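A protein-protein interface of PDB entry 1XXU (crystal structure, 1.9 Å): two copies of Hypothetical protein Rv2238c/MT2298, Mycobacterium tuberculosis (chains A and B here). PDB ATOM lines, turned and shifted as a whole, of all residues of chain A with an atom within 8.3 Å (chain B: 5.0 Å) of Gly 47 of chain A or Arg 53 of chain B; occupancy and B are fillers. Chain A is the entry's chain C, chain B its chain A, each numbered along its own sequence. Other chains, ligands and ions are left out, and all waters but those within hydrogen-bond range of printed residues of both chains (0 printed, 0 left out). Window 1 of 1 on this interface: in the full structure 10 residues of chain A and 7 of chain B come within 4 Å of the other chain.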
ATOM      1  N   THR A  42      25.213  18.527  -7.050  1.00  0.00           N
ATOM      2  CA  THR A  42      25.140  19.747  -7.860  1.00  0.00           C
ATOM      3  C   THR A  42      23.727  20.271  -7.699  1.00  0.00           C
ATOM      4  O   THR A  42      22.818  19.532  -7.331  1.00  0.00           O
ATOM      5  CB  THR A  42      25.521  19.545  -9.364  1.00  0.00           C
ATOM      6  OG1 THR A  42      24.632  18.621  -9.994  1.00  0.00           O
ATOM      7  CG2 THR A  42      26.959  19.035  -9.468  1.00  0.00           C
ATOM      8  N   GLY A  43      23.564  21.563  -7.931  1.00  0.00           N
ATOM      9  CA  GLY A  43      22.276  22.195  -7.752  1.00  0.00           C
ATOM     10  C   GLY A  43      21.071  21.710  -8.545  1.00  0.00           C
ATOM     11  O   GLY A  43      20.052  21.343  -7.948  1.00  0.00           O
ATOM     12  N   ILE A  44      21.155  21.709  -9.869  1.00  0.00           N
ATOM     13  CA  ILE A  44      19.982  21.295 -10.632  1.00  0.00           C
ATOM     14  C   ILE A  44      19.648  19.820 -10.383  1.00  0.00           C
ATOM     15  O   ILE A  44      18.476  19.450 -10.269  1.00  0.00           O
ATOM     16  CB  ILE A  44      20.156  21.580 -12.124  1.00  0.00           C
ATOM     17  CG1 ILE A  44      20.258  23.101 -12.339  1.00  0.00           C
ATOM     18  CG2 ILE A  44      18.960  21.013 -12.920  1.00  0.00           C
ATOM     19  CD1 ILE A  44      20.637  23.468 -13.774  1.00  0.00           C
ATOM     20  N   CYS A  45      20.674  18.986 -10.253  1.00  0.00           N
ATOM     21  CA  CYS A  45      20.443  17.570  -9.971  1.00  0.00           C
ATOM     22  C   CYS A  45      19.740  17.431  -8.621  1.00  0.00           C
ATOM     23  O   CYS A  45      18.856  16.600  -8.449  1.00  0.00           O
ATOM     24  CB  CYS A  45      21.776  16.803  -9.954  1.00  0.00           C
ATOM     25  SG  CYS A  45      22.605  16.657 -11.555  1.00  0.00           S
ATOM     26  N   GLN A  46      20.134  18.251  -7.657  1.00  0.00           N
ATOM     27  CA  GLN A  46      19.545  18.219  -6.318  1.00  0.00           C
ATOM     28  C   GLN A  46      18.054  18.523  -6.431  1.00  0.00           C
ATOM     29  O   GLN A  46      17.222  17.822  -5.867  1.00  0.00           O
ATOM     30  CB  GLN A  46      20.231  19.262  -5.415  1.00  0.00           C
ATOM     31  CG  GLN A  46      19.779  19.260  -3.942  1.00  0.00           C
ATOM     32  CD  GLN A  46      20.349  18.120  -3.107  1.00  0.00           C
ATOM     33  OE1 GLN A  46      19.611  17.263  -2.655  1.00  0.00           O
ATOM     34  NE2 GLN A  46      21.644  18.132  -2.870  1.00  0.00           N
ATOM     35  N   GLY A  47      17.727  19.572  -7.181  1.00  0.00           N
ATOM     36  CA  GLY A  47      16.347  19.964  -7.371  1.00  0.00           C
ATOM     37  C   GLY A  47      15.505  18.899  -8.065  1.00  0.00           C
ATOM     38  O   GLY A  47      14.368  18.619  -7.686  1.00  0.00           O
ATOM     39  N   GLU A  48      16.056  18.291  -9.100  1.00  0.00           N
ATOM     40  CA  GLU A  48      15.307  17.273  -9.807  1.00  0.00           C
ATOM     41  C   GLU A  48      15.022  16.085  -8.901  1.00  0.00           C
ATOM     42  O   GLU A  48      13.866  15.626  -8.805  1.00  0.00           O
ATOM     43  CB  GLU A  48      16.085  16.817 -11.049  1.00  0.00           C
ATOM     44  CG  GLU A  48      16.157  17.877 -12.114  1.00  0.00           C
ATOM     45  CD  GLU A  48      16.546  17.296 -13.445  1.00  0.00           C
ATOM     46  OE1 GLU A  48      15.755  17.454 -14.401  1.00  0.00           O
ATOM     47  OE2 GLU A  48      17.637  16.687 -13.517  1.00  0.00           O
ATOM     48  N   LEU A  49      16.061  15.612  -8.209  1.00  0.00           N
ATOM     49  CA  LEU A  49      15.894  14.455  -7.340  1.00  0.00           C
ATOM     50  C   LEU A  49      15.101  14.747  -6.071  1.00  0.00           C
ATOM     51  O   LEU A  49      14.488  13.847  -5.524  1.00  0.00           O
ATOM     52  CB  LEU A  49      17.247  13.829  -7.009  1.00  0.00           C
ATOM     53  CG  LEU A  49      18.089  13.267  -8.162  1.00  0.00           C
ATOM     54  CD1 LEU A  49      19.011  12.191  -7.579  1.00  0.00           C
ATOM     55  CD2 LEU A  49      17.224  12.688  -9.294  1.00  0.00           C
ATOM     56  N   ASP A  50      15.113  15.991  -5.598  1.00  0.00           N
ATOM     57  CA  ASP A  50      14.302  16.333  -4.427  1.00  0.00           C
ATOM     58  C   ASP A  50      12.837  16.253  -4.897  1.00  0.00           C
ATOM     59  O   ASP A  50      11.952  15.850  -4.152  1.00  0.00           O
ATOM     60  CB  ASP A  50      14.594  17.756  -3.931  1.00  0.00           C
ATOM     61  CG  ASP A  50      15.882  17.845  -3.123  1.00  0.00           C
ATOM     62  OD1 ASP A  50      16.618  16.844  -3.044  1.00  0.00           O
ATOM     63  OD2 ASP A  50      16.160  18.927  -2.556  1.00  0.00           O
ATOM     64  N   GLN A  51      12.594  16.648  -6.146  1.00  0.00           N
ATOM     65  CA  GLN A  51      11.230  16.602  -6.688  1.00  0.00           C
ATOM     66  C   GLN A  51      10.776  15.150  -6.801  1.00  0.00           C
ATOM     67  O   GLN A  51       9.634  14.804  -6.477  1.00  0.00           O
ATOM     68  CB  GLN A  51      11.159  17.237  -8.081  1.00  0.00           C
ATOM     69  CG  GLN A  51      11.140  18.728  -8.096  1.00  0.00           C
ATOM     70  CD  GLN A  51      10.619  19.279  -9.424  1.00  0.00           C
ATOM     71  OE1 GLN A  51      10.924  20.417  -9.793  1.00  0.00           O
ATOM     72  NE2 GLN A  51       9.814  18.479 -10.136  1.00  0.00           N
ATOM     73  N   LEU A  52      11.684  14.293  -7.250  1.00  0.00           N
ATOM     74  CA  LEU A  52      11.348  12.878  -7.391  1.00  0.00           C
ATOM     75  C   LEU A  52      11.015  12.334  -5.999  1.00  0.00           C
ATOM     76  O   LEU A  52      10.005  11.645  -5.805  1.00  0.00           O
ATOM     77  CB  LEU A  52      12.531  12.119  -8.013  1.00  0.00           C
ATOM     78  CG  LEU A  52      12.301  10.762  -8.686  1.00  0.00           C
ATOM     79  CD1 LEU A  52      11.175  10.842  -9.697  1.00  0.00           C
ATOM     80  CD2 LEU A  52      13.579  10.360  -9.417  1.00  0.00           C
ATOM     81  N   ARG A  53      11.881  12.662  -5.047  1.00  0.00           N
ATOM     82  CA  ARG A  53      11.744  12.255  -3.650  1.00  0.00           C
ATOM     83  C   ARG A  53      10.389  12.693  -3.082  1.00  0.00           C
ATOM     84  O   ARG A  53       9.670  11.910  -2.424  1.00  0.00           O
ATOM     85  CB  ARG A  53      12.875  12.906  -2.834  1.00  0.00           C
ATOM     86  CG  ARG A  53      12.782  12.716  -1.323  1.00  0.00           C
ATOM     87  CD  ARG A  53      13.689  13.735  -0.606  1.00  0.00           C
ATOM     88  NE  ARG A  53      13.171  15.102  -0.727  1.00  0.00           N
ATOM     89  CZ  ARG A  53      13.855  16.205  -0.424  1.00  0.00           C
ATOM     90  NH1 ARG A  53      15.100  16.120   0.027  1.00  0.00           N
ATOM     91  NH2 ARG A  53      13.297  17.403  -0.597  1.00  0.00           N
ATOM     92  N   ASP A  54      10.048  13.951  -3.350  1.00  0.00           N
ATOM     93  CA  ASP A  54       8.811  14.524  -2.849  1.00  0.00           C
ATOM     94  C   ASP A  54       7.543  13.880  -3.438  1.00  0.00           C
ATOM     95  O   ASP A  54       6.464  13.950  -2.850  1.00  0.00           O
ATOM     96  CB  ASP A  54       8.820  16.038  -3.102  1.00  0.00           C
ATOM     97  CG  ASP A  54       9.807  16.781  -2.202  1.00  0.00           C
ATOM     98  OD1 ASP A  54      10.428  16.149  -1.330  1.00  0.00           O
ATOM     99  OD2 ASP A  54       9.956  18.009  -2.353  1.00  0.00           O
ATOM    100  N   HIS A  55       7.689  13.236  -4.586  1.00  0.00           N
ATOM    101  CA  HIS A  55       6.579  12.589  -5.268  1.00  0.00           C
ATOM    102  C   HIS A  55       6.857  11.110  -5.540  1.00  0.00           C
ATOM    103  O   HIS A  55       6.247  10.522  -6.438  1.00  0.00           O
ATOM    104  CB  HIS A  55       6.345  13.303  -6.594  1.00  0.00           C
ATOM    105  CG  HIS A  55       5.941  14.737  -6.441  1.00  0.00           C
ATOM    106  ND1 HIS A  55       4.638  15.119  -6.197  1.00  0.00           N
ATOM    107  CD2 HIS A  55       6.673  15.877  -6.445  1.00  0.00           C
ATOM    108  CE1 HIS A  55       4.586  16.432  -6.057  1.00  0.00           C
ATOM    109  NE2 HIS A  55       5.807  16.917  -6.201  1.00  0.00           N
ATOM    110  N   TRP A  80      25.269  11.348  -0.474  1.00  0.00           N
ATOM    111  CA  TRP A  80      24.298  12.288  -0.995  1.00  0.00           C
ATOM    112  C   TRP A  80      22.866  11.820  -0.695  1.00  0.00           C
ATOM    113  O   TRP A  80      22.030  12.616  -0.258  1.00  0.00           O
ATOM    114  CB  TRP A  80      24.528  12.478  -2.491  1.00  0.00           C
ATOM    115  CG  TRP A  80      23.773  13.633  -3.065  1.00  0.00           C
ATOM    116  CD1 TRP A  80      23.610  14.867  -2.497  1.00  0.00           C
ATOM    117  CD2 TRP A  80      23.118  13.684  -4.339  1.00  0.00           C
ATOM    118  NE1 TRP A  80      22.891  15.683  -3.347  1.00  0.00           N
ATOM    119  CE2 TRP A  80      22.576  14.980  -4.480  1.00  0.00           C
ATOM    120  CE3 TRP A  80      22.939  12.755  -5.380  1.00  0.00           C
ATOM    121  CZ2 TRP A  80      21.862  15.378  -5.626  1.00  0.00           C
ATOM    122  CZ3 TRP A  80      22.240  13.137  -6.507  1.00  0.00           C
ATOM    123  CH2 TRP A  80      21.701  14.444  -6.627  1.00  0.00           C
ATOM    124  N   SER A  84      20.270  13.706   1.645  1.00  0.00           N
ATOM    125  CA  SER A  84      19.113  14.195   0.911  1.00  0.00           C
ATOM    126  C   SER A  84      17.801  13.449   1.201  1.00  0.00           C
ATOM    127  O   SER A  84      16.738  13.895   0.789  1.00  0.00           O
ATOM    128  CB  SER A  84      19.420  14.161  -0.591  1.00  0.00           C
ATOM    129  OG  SER A  84      20.593  14.913  -0.907  1.00  0.00           O
ATOM    130  N   PHE A  86      17.067  10.420   0.106  1.00  0.00           N
ATOM    131  CA  PHE A  86      16.691   9.674  -1.110  1.00  0.00           C
ATOM    132  C   PHE A  86      16.614   8.202  -0.763  1.00  0.00           C
ATOM    133  O   PHE A  86      17.624   7.633  -0.358  1.00  0.00           O
ATOM    134  CB  PHE A  86      17.746   9.827  -2.221  1.00  0.00           C
ATOM    135  CG  PHE A  86      17.897  11.216  -2.752  1.00  0.00           C
ATOM    136  CD1 PHE A  86      16.866  12.165  -2.639  1.00  0.00           C
ATOM    137  CD2 PHE A  86      19.081  11.592  -3.378  1.00  0.00           C
ATOM    138  CE1 PHE A  86      17.022  13.454  -3.135  1.00  0.00           C
ATOM    139  CE2 PHE A  86      19.251  12.895  -3.883  1.00  0.00           C
ATOM    140  CZ  PHE A  86      18.215  13.833  -3.760  1.00  0.00           C
ATOM    141  N   ARG A 116      21.045  14.981 -19.079  1.00  0.00           N
ATOM    142  CA  ARG A 116      19.778  14.709 -18.380  1.00  0.00           C
ATOM    143  C   ARG A 116      18.857  13.866 -19.257  1.00  0.00           C
ATOM    144  O   ARG A 116      17.867  14.351 -19.810  1.00  0.00           O
ATOM    145  CB  ARG A 116      19.091  16.017 -17.997  1.00  0.00           C
ATOM    146  CG  ARG A 116      19.998  16.878 -17.132  1.00  0.00           C
ATOM    147  CD  ARG A 116      19.302  18.070 -16.492  1.00  0.00           C
ATOM    148  NE  ARG A 116      20.316  18.846 -15.788  1.00  0.00           N
ATOM    149  CZ  ARG A 116      20.801  18.543 -14.590  1.00  0.00           C
ATOM    150  NH1 ARG A 116      21.756  19.300 -14.046  1.00  0.00           N
ATOM    151  NH2 ARG A 116      20.317  17.510 -13.916  1.00  0.00           N
ATOM    152  N   VAL A 138      16.418  22.053 -17.169  1.00  0.00           N
ATOM    153  CA  VAL A 138      15.616  21.350 -16.177  1.00  0.00           C
ATOM    154  C   VAL A 138      14.504  20.544 -16.856  1.00  0.00           C
ATOM    155  O   VAL A 138      13.930  20.976 -17.866  1.00  0.00           O
ATOM    156  CB  VAL A 138      15.020  22.371 -15.171  1.00  0.00           C
ATOM    157  CG1 VAL A 138      14.272  21.644 -14.044  1.00  0.00           C
ATOM    158  CG2 VAL A 138      16.148  23.238 -14.611  1.00  0.00           C
ATOM    159  N   ARG A 139      14.211  19.368 -16.317  1.00  0.00           N
ATOM    160  CA  ARG A 139      13.188  18.502 -16.909  1.00  0.00           C
ATOM    161  C   ARG A 139      11.785  18.721 -16.350  1.00  0.00           C
ATOM    162  O   ARG A 139      11.624  19.158 -15.222  1.00  0.00           O
ATOM    163  CB  ARG A 139      13.593  17.024 -16.719  1.00  0.00           C
ATOM    164  CG  ARG A 139      14.602  16.542 -17.723  1.00  0.00           C
ATOM    165  CD  ARG A 139      15.149  15.139 -17.384  1.00  0.00           C
ATOM    166  NE  ARG A 139      16.069  15.199 -16.249  1.00  0.00           N
ATOM    167  CZ  ARG A 139      16.938  14.244 -15.941  1.00  0.00           C
ATOM    168  NH1 ARG A 139      17.010  13.133 -16.688  1.00  0.00           N
ATOM    169  NH2 ARG A 139      17.733  14.412 -14.887  1.00  0.00           N
ATOM    170  N   GLN A 141       8.845  16.870 -15.046  1.00  0.00           N
ATOM    171  CA  GLN A 141       8.509  15.578 -14.486  1.00  0.00           C
ATOM    172  C   GLN A 141       7.074  15.110 -14.703  1.00  0.00           C
ATOM    173  O   GLN A 141       6.753  13.963 -14.405  1.00  0.00           O
ATOM    174  CB  GLN A 141       8.865  15.575 -13.001  1.00  0.00           C
ATOM    175  CG  GLN A 141      10.381  15.656 -12.788  1.00  0.00           C
ATOM    176  CD  GLN A 141      10.810  15.352 -11.367  1.00  0.00           C
ATOM    177  OE1 GLN A 141      10.061  14.762 -10.579  1.00  0.00           O
ATOM    178  NE2 GLN A 141      12.027  15.745 -11.037  1.00  0.00           N
ATOM    179  N   TRP A 144       7.069  12.564 -17.174  1.00  0.00           N
ATOM    180  CA  TRP A 144       7.471  11.268 -16.634  1.00  0.00           C
ATOM    181  C   TRP A 144       6.253  10.484 -16.123  1.00  0.00           C
ATOM    182  O   TRP A 144       6.020   9.342 -16.542  1.00  0.00           O
ATOM    183  CB  TRP A 144       8.472  11.448 -15.501  1.00  0.00           C
ATOM    184  CG  TRP A 144       9.757  12.200 -15.854  1.00  0.00           C
ATOM    185  CD1 TRP A 144      10.149  12.686 -17.080  1.00  0.00           C
ATOM    186  CD2 TRP A 144      10.802  12.535 -14.939  1.00  0.00           C
ATOM    187  NE1 TRP A 144      11.386  13.300 -16.974  1.00  0.00           N
ATOM    188  CE2 TRP A 144      11.807  13.216 -15.670  1.00  0.00           C
ATOM    189  CE3 TRP A 144      10.988  12.327 -13.564  1.00  0.00           C
ATOM    190  CZ2 TRP A 144      12.989  13.684 -15.061  1.00  0.00           C
ATOM    191  CZ3 TRP A 144      12.164  12.794 -12.958  1.00  0.00           C
ATOM    192  CH2 TRP A 144      13.144  13.459 -13.702  1.00  0.00           C
ATOM    193  N   LEU B  49      15.301  29.611  -0.792  1.00  0.00           N
ATOM    194  CA  LEU B  49      15.394  29.501  -2.247  1.00  0.00           C
ATOM    195  C   LEU B  49      15.560  28.045  -2.713  1.00  0.00           C
ATOM    196  O   LEU B  49      15.196  27.686  -3.854  1.00  0.00           O
ATOM    197  CB  LEU B  49      16.537  30.370  -2.762  1.00  0.00           C
ATOM    198  CG  LEU B  49      16.332  31.890  -2.607  1.00  0.00           C
ATOM    199  CD1 LEU B  49      17.402  32.641  -3.405  1.00  0.00           C
ATOM    200  CD2 LEU B  49      14.972  32.272  -3.163  1.00  0.00           C
ATOM    201  N   ASP B  50      16.139  27.224  -1.843  1.00  0.00           N
ATOM    202  CA  ASP B  50      16.288  25.800  -2.118  1.00  0.00           C
ATOM    203  C   ASP B  50      14.871  25.202  -2.166  1.00  0.00           C
ATOM    204  O   ASP B  50      14.595  24.335  -2.978  1.00  0.00           O
ATOM    205  CB  ASP B  50      17.092  25.098  -1.012  1.00  0.00           C
ATOM    206  CG  ASP B  50      18.566  25.428  -1.066  1.00  0.00           C
ATOM    207  OD1 ASP B  50      18.990  26.036  -2.061  1.00  0.00           O
ATOM    208  OD2 ASP B  50      19.302  25.077  -0.112  1.00  0.00           O
ATOM    209  N   GLN B  51      13.982  25.668  -1.294  1.00  0.00           N
ATOM    210  CA  GLN B  51      12.601  25.158  -1.297  1.00  0.00           C
ATOM    211  C   GLN B  51      11.966  25.547  -2.624  1.00  0.00           C
ATOM    212  O   GLN B  51      11.312  24.743  -3.259  1.00  0.00           O
ATOM    213  CB  GLN B  51      11.741  25.772  -0.184  1.00  0.00           C
ATOM    214  CG  GLN B  51      12.222  25.625   1.237  1.00  0.00           C
ATOM    215  CD  GLN B  51      11.275  26.333   2.202  1.00  0.00           C
ATOM    216  OE1 GLN B  51      11.709  27.082   3.099  1.00  0.00           O
ATOM    217  NE2 GLN B  51       9.966  26.109   2.014  1.00  0.00           N
ATOM    218  N   LEU B  52      12.147  26.805  -3.012  1.00  0.00           N
ATOM    219  CA  LEU B  52      11.612  27.331  -4.261  1.00  0.00           C
ATOM    220  C   LEU B  52      12.109  26.528  -5.456  1.00  0.00           C
ATOM    221  O   LEU B  52      11.326  26.164  -6.329  1.00  0.00           O
ATOM    222  CB  LEU B  52      12.003  28.806  -4.388  1.00  0.00           C
ATOM    223  CG  LEU B  52      11.798  29.588  -5.697  1.00  0.00           C
ATOM    224  CD1 LEU B  52      10.563  29.153  -6.433  1.00  0.00           C
ATOM    225  CD2 LEU B  52      11.720  31.101  -5.336  1.00  0.00           C
ATOM    226  N   ARG B  53      13.409  26.242  -5.490  1.00  0.00           N
ATOM    227  CA  ARG B  53      13.999  25.426  -6.571  1.00  0.00           C
ATOM    228  C   ARG B  53      13.307  24.051  -6.619  1.00  0.00           C
ATOM    229  O   ARG B  53      12.902  23.574  -7.673  1.00  0.00           O
ATOM    230  CB  ARG B  53      15.486  25.211  -6.296  1.00  0.00           C
ATOM    231  CG  ARG B  53      16.172  24.171  -7.191  1.00  0.00           C
ATOM    232  CD  ARG B  53      17.497  23.726  -6.567  1.00  0.00           C
ATOM    233  NE  ARG B  53      17.237  23.053  -5.303  1.00  0.00           N
ATOM    234  CZ  ARG B  53      18.114  22.889  -4.318  1.00  0.00           C
ATOM    235  NH1 ARG B  53      19.349  23.360  -4.436  1.00  0.00           N
ATOM    236  NH2 ARG B  53      17.752  22.223  -3.214  1.00  0.00           N
ATOM    237  N   ASP B  54      13.192  23.412  -5.459  1.00  0.00           N
ATOM    238  CA  ASP B  54      12.565  22.096  -5.377  1.00  0.00           C
ATOM    239  C   ASP B  54      11.073  22.078  -5.743  1.00  0.00           C
ATOM    240  O   ASP B  54      10.510  21.012  -6.044  1.00  0.00           O
ATOM    241  CB  ASP B  54      12.719  21.529  -3.971  1.00  0.00           C
ATOM    242  CG  ASP B  54      14.145  21.173  -3.635  1.00  0.00           C
ATOM    243  OD1 ASP B  54      15.045  21.445  -4.439  1.00  0.00           O
ATOM    244  OD2 ASP B  54      14.359  20.617  -2.546  1.00  0.00           O
ATOM    245  N   HIS B  55      10.424  23.231  -5.674  1.00  0.00           N
ATOM    246  CA  HIS B  55       8.998  23.305  -6.026  1.00  0.00           C
ATOM    247  C   HIS B  55       8.758  24.242  -7.221  1.00  0.00           C
ATOM    248  O   HIS B  55       7.644  24.719  -7.425  1.00  0.00           O
ATOM    249  CB  HIS B  55       8.190  23.788  -4.799  1.00  0.00           C
ATOM    250  CG  HIS B  55       8.194  22.806  -3.665  1.00  0.00           C
ATOM    251  ND1 HIS B  55       7.276  21.779  -3.570  1.00  0.00           N
ATOM    252  CD2 HIS B  55       9.059  22.632  -2.635  1.00  0.00           C
ATOM    253  CE1 HIS B  55       7.572  21.017  -2.530  1.00  0.00           C
ATOM    254  NE2 HIS B  55       8.649  21.513  -1.944  1.00  0.00           N
ATOM    255  N   LEU B  56       9.788  24.451  -8.039  1.00  0.00           N
ATOM    256  CA  LEU B  56       9.689  25.398  -9.153  1.00  0.00           C
ATOM    257  C   LEU B  56       8.473  25.331 -10.072  1.00  0.00           C
ATOM    258  O   LEU B  56       8.023  26.369 -10.508  1.00  0.00           O
ATOM    259  CB  LEU B  56      10.973  25.394  -9.999  1.00  0.00           C
ATOM    260  CG  LEU B  56      11.237  26.655 -10.859  1.00  0.00           C
ATOM    261  CD1 LEU B  56      11.008  27.946 -10.045  1.00  0.00           C
ATOM    262  CD2 LEU B  56      12.685  26.616 -11.365  1.00  0.00           C
ATOM    263  N   SER B  84      23.831  26.746  -6.528  1.00  0.00           N
ATOM    264  CA  SER B  84      22.603  26.291  -5.851  1.00  0.00           C
ATOM    265  C   SER B  84      21.494  25.645  -6.700  1.00  0.00           C
ATOM    266  O   SER B  84      20.536  25.077  -6.142  1.00  0.00           O
ATOM    267  CB  SER B  84      21.967  27.460  -5.107  1.00  0.00           C
ATOM    268  OG  SER B  84      22.830  27.968  -4.118  1.00  0.00           O
ATOM    269  N   GLY B  85      21.607  25.743  -8.022  1.00  0.00           N
ATOM    270  CA  GLY B  85      20.590  25.186  -8.890  1.00  0.00           C
ATOM    271  C   GLY B  85      19.387  26.111  -9.058  1.00  0.00           C
ATOM    272  O   GLY B  85      18.235  25.650  -9.270  1.00  0.00           O
ATOM    273  N   PHE B  86      19.633  27.417  -8.960  1.00  0.00           N
ATOM    274  CA  PHE B  86      18.564  28.394  -9.119  1.00  0.00           C
ATOM    275  C   PHE B  86      18.394  28.753 -10.595  1.00  0.00           C
ATOM    276  O   PHE B  86      19.086  29.603 -11.130  1.00  0.00           O
ATOM    277  CB  PHE B  86      18.848  29.656  -8.271  1.00  0.00           C
ATOM    278  CG  PHE B  86      18.979  29.376  -6.779  1.00  0.00           C
ATOM    279  CD1 PHE B  86      18.444  28.209  -6.218  1.00  0.00           C
ATOM    280  CD2 PHE B  86      19.619  30.288  -5.945  1.00  0.00           C
ATOM    281  CE1 PHE B  86      18.560  27.971  -4.832  1.00  0.00           C
ATOM    282  CE2 PHE B  86      19.742  30.060  -4.569  1.00  0.00           C
ATOM    283  CZ  PHE B  86      19.214  28.898  -4.013  1.00  0.00           C
ATOM    284  N   PHE B  88      15.707  30.045 -11.882  1.00  0.00           N
ATOM    285  CA  PHE B  88      14.742  31.131 -11.977  1.00  0.00           C
ATOM    286  C   PHE B  88      15.531  32.426 -11.799  1.00  0.00           C
ATOM    287  O   PHE B  88      16.692  32.402 -11.346  1.00  0.00           O
ATOM    288  CB  PHE B  88      13.691  31.007 -10.866  1.00  0.00           C
ATOM    289  CG  PHE B  88      14.287  30.806  -9.501  1.00  0.00           C
ATOM    290  CD1 PHE B  88      14.744  31.880  -8.759  1.00  0.00           C
ATOM    291  CD2 PHE B  88      14.395  29.521  -8.967  1.00  0.00           C
ATOM    292  CE1 PHE B  88      15.300  31.687  -7.496  1.00  0.00           C
ATOM    293  CE2 PHE B  88      14.954  29.317  -7.695  1.00  0.00           C
ATOM    294  CZ  PHE B  88      15.399  30.397  -6.966  1.00  0.00           C
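Asp 50 of chain A touches Arg 53 of chain B, but with the chains exchanged Arg 53 of chain A does not touch Asp 50 of chain B (7.4 Å). Asp 50 of chain A touches Asp 54 of chain B, but with the chains exchanged Asp 54 of chain A does not touch Asp 50 of chain B (7.9 Å). Gln 51 of chain A touches Asp 54 of chain B, but with the chains exchanged Asp 54 of chain A does not touch Gln 51 of chain B (6.9 Å). Asp 54 of chain A touches His 55 of chain B, but with the chains exchanged His 55 of chain A does not touch Asp 54 of chain B (6.2 Å). Of the 12 pairs that touch across the chains among the printed residues, none has its exchanged pair printed and touching as well.
Printed residues of chain B that touch a printed residue of chain A: Arg 53, Asp 54, His 55, Ser 84 and Gly 85. Along chain B the printed residues that touch a printed residue of chain A span positions 53 to 85. Among the printed residues, Asp or Glu carboxylates within 4 Å of a Lys or Arg side-chain nitrogen of the other chain: Asp 50 of chain A with Arg 53 of chain B and Arg 53 of chain A with Asp 54 of chain B.
The side-chain hydroxyl (OG) of Ser 84 of chain A sits at hydrogen-bond distance from the side-chain amide oxygen (OE1) of Gln 46 of chain A, 3.1 Å away. The side-chain carboxylate (OD1) of Asp 50 of chain A lies within salt-bridge range of the guanidinium group (NH1) of Arg 53 of chain A (3.5 Å). The side-chain amide nitrogen (NE2) of Gln 46 of chain A lies close to the indole nitrogen (NE1) of Trp 80 of chain A (2.8 Å). The side-chain carboxylate of Asp 50 of chain B is in salt-bridge range of the guanidinium group of Arg 53 of chain B (3.6 Å). OD1 of Asp 54 of chain B is in salt-bridge range of NE of Arg 53 of chain B. The guanidinium group of Arg 53 of chain B is in hydrogen-bond range of the backbone carbonyl oxygen of Ser 84 of chain B, at 2.7 Å.
Of the printed residues of chain B, Gln 46 of chain A touches Arg 53. Of the printed residues of chain B, Asp 54 of chain A touches His 55. Arg 53 of chain B touches four residues of chain A. Asp 54 of chain B touches four residues of chain A. The nearest residue of chain A that does not touch Arg 53 of chain B is Gln 51 of chain A (4.3 Å). The nearest printed residue of chain B that does not touch Gln 51 of chain A is Arg 53 of chain B (4.3 Å).
Among the printed residues, merely in contact across the chains: Gln 51 of chain A with Asp 54 of chain B (3.1 Å), Gly 43 of chain A with Gly 85 of chain B (3.5 Å), Gly 47 of chain A with Asp 54 of chain B (3.5 Å), Ile 44 of chain A with Gly 85 of chain B (3.7 Å), Gln 46 of chain A with Arg 53 of chain B (3.7 Å), Gly 43 of chain A with Ser 84 of chain B (3.7 Å), Gly 43 of chain A with Arg 53 of chain B (3.8 Å), Asp 54 of chain A with His 55 of chain B (3.8 Å) and Gly 47 of chain A with Arg 53 of chain B (3.8 Å).
OD2 of Asp 54 of chain B lies close to OD2 of Asp 50 of chain A, at 2.5 Å. OD2 of Asp 54 of chain B is in salt-bridge range of NH2 of Arg 53 of chain A (3.9 Å). NH2 of Arg 53 of chain B lies within salt-bridge range of OD2 of Asp 50 of chain A (3.7 Å).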
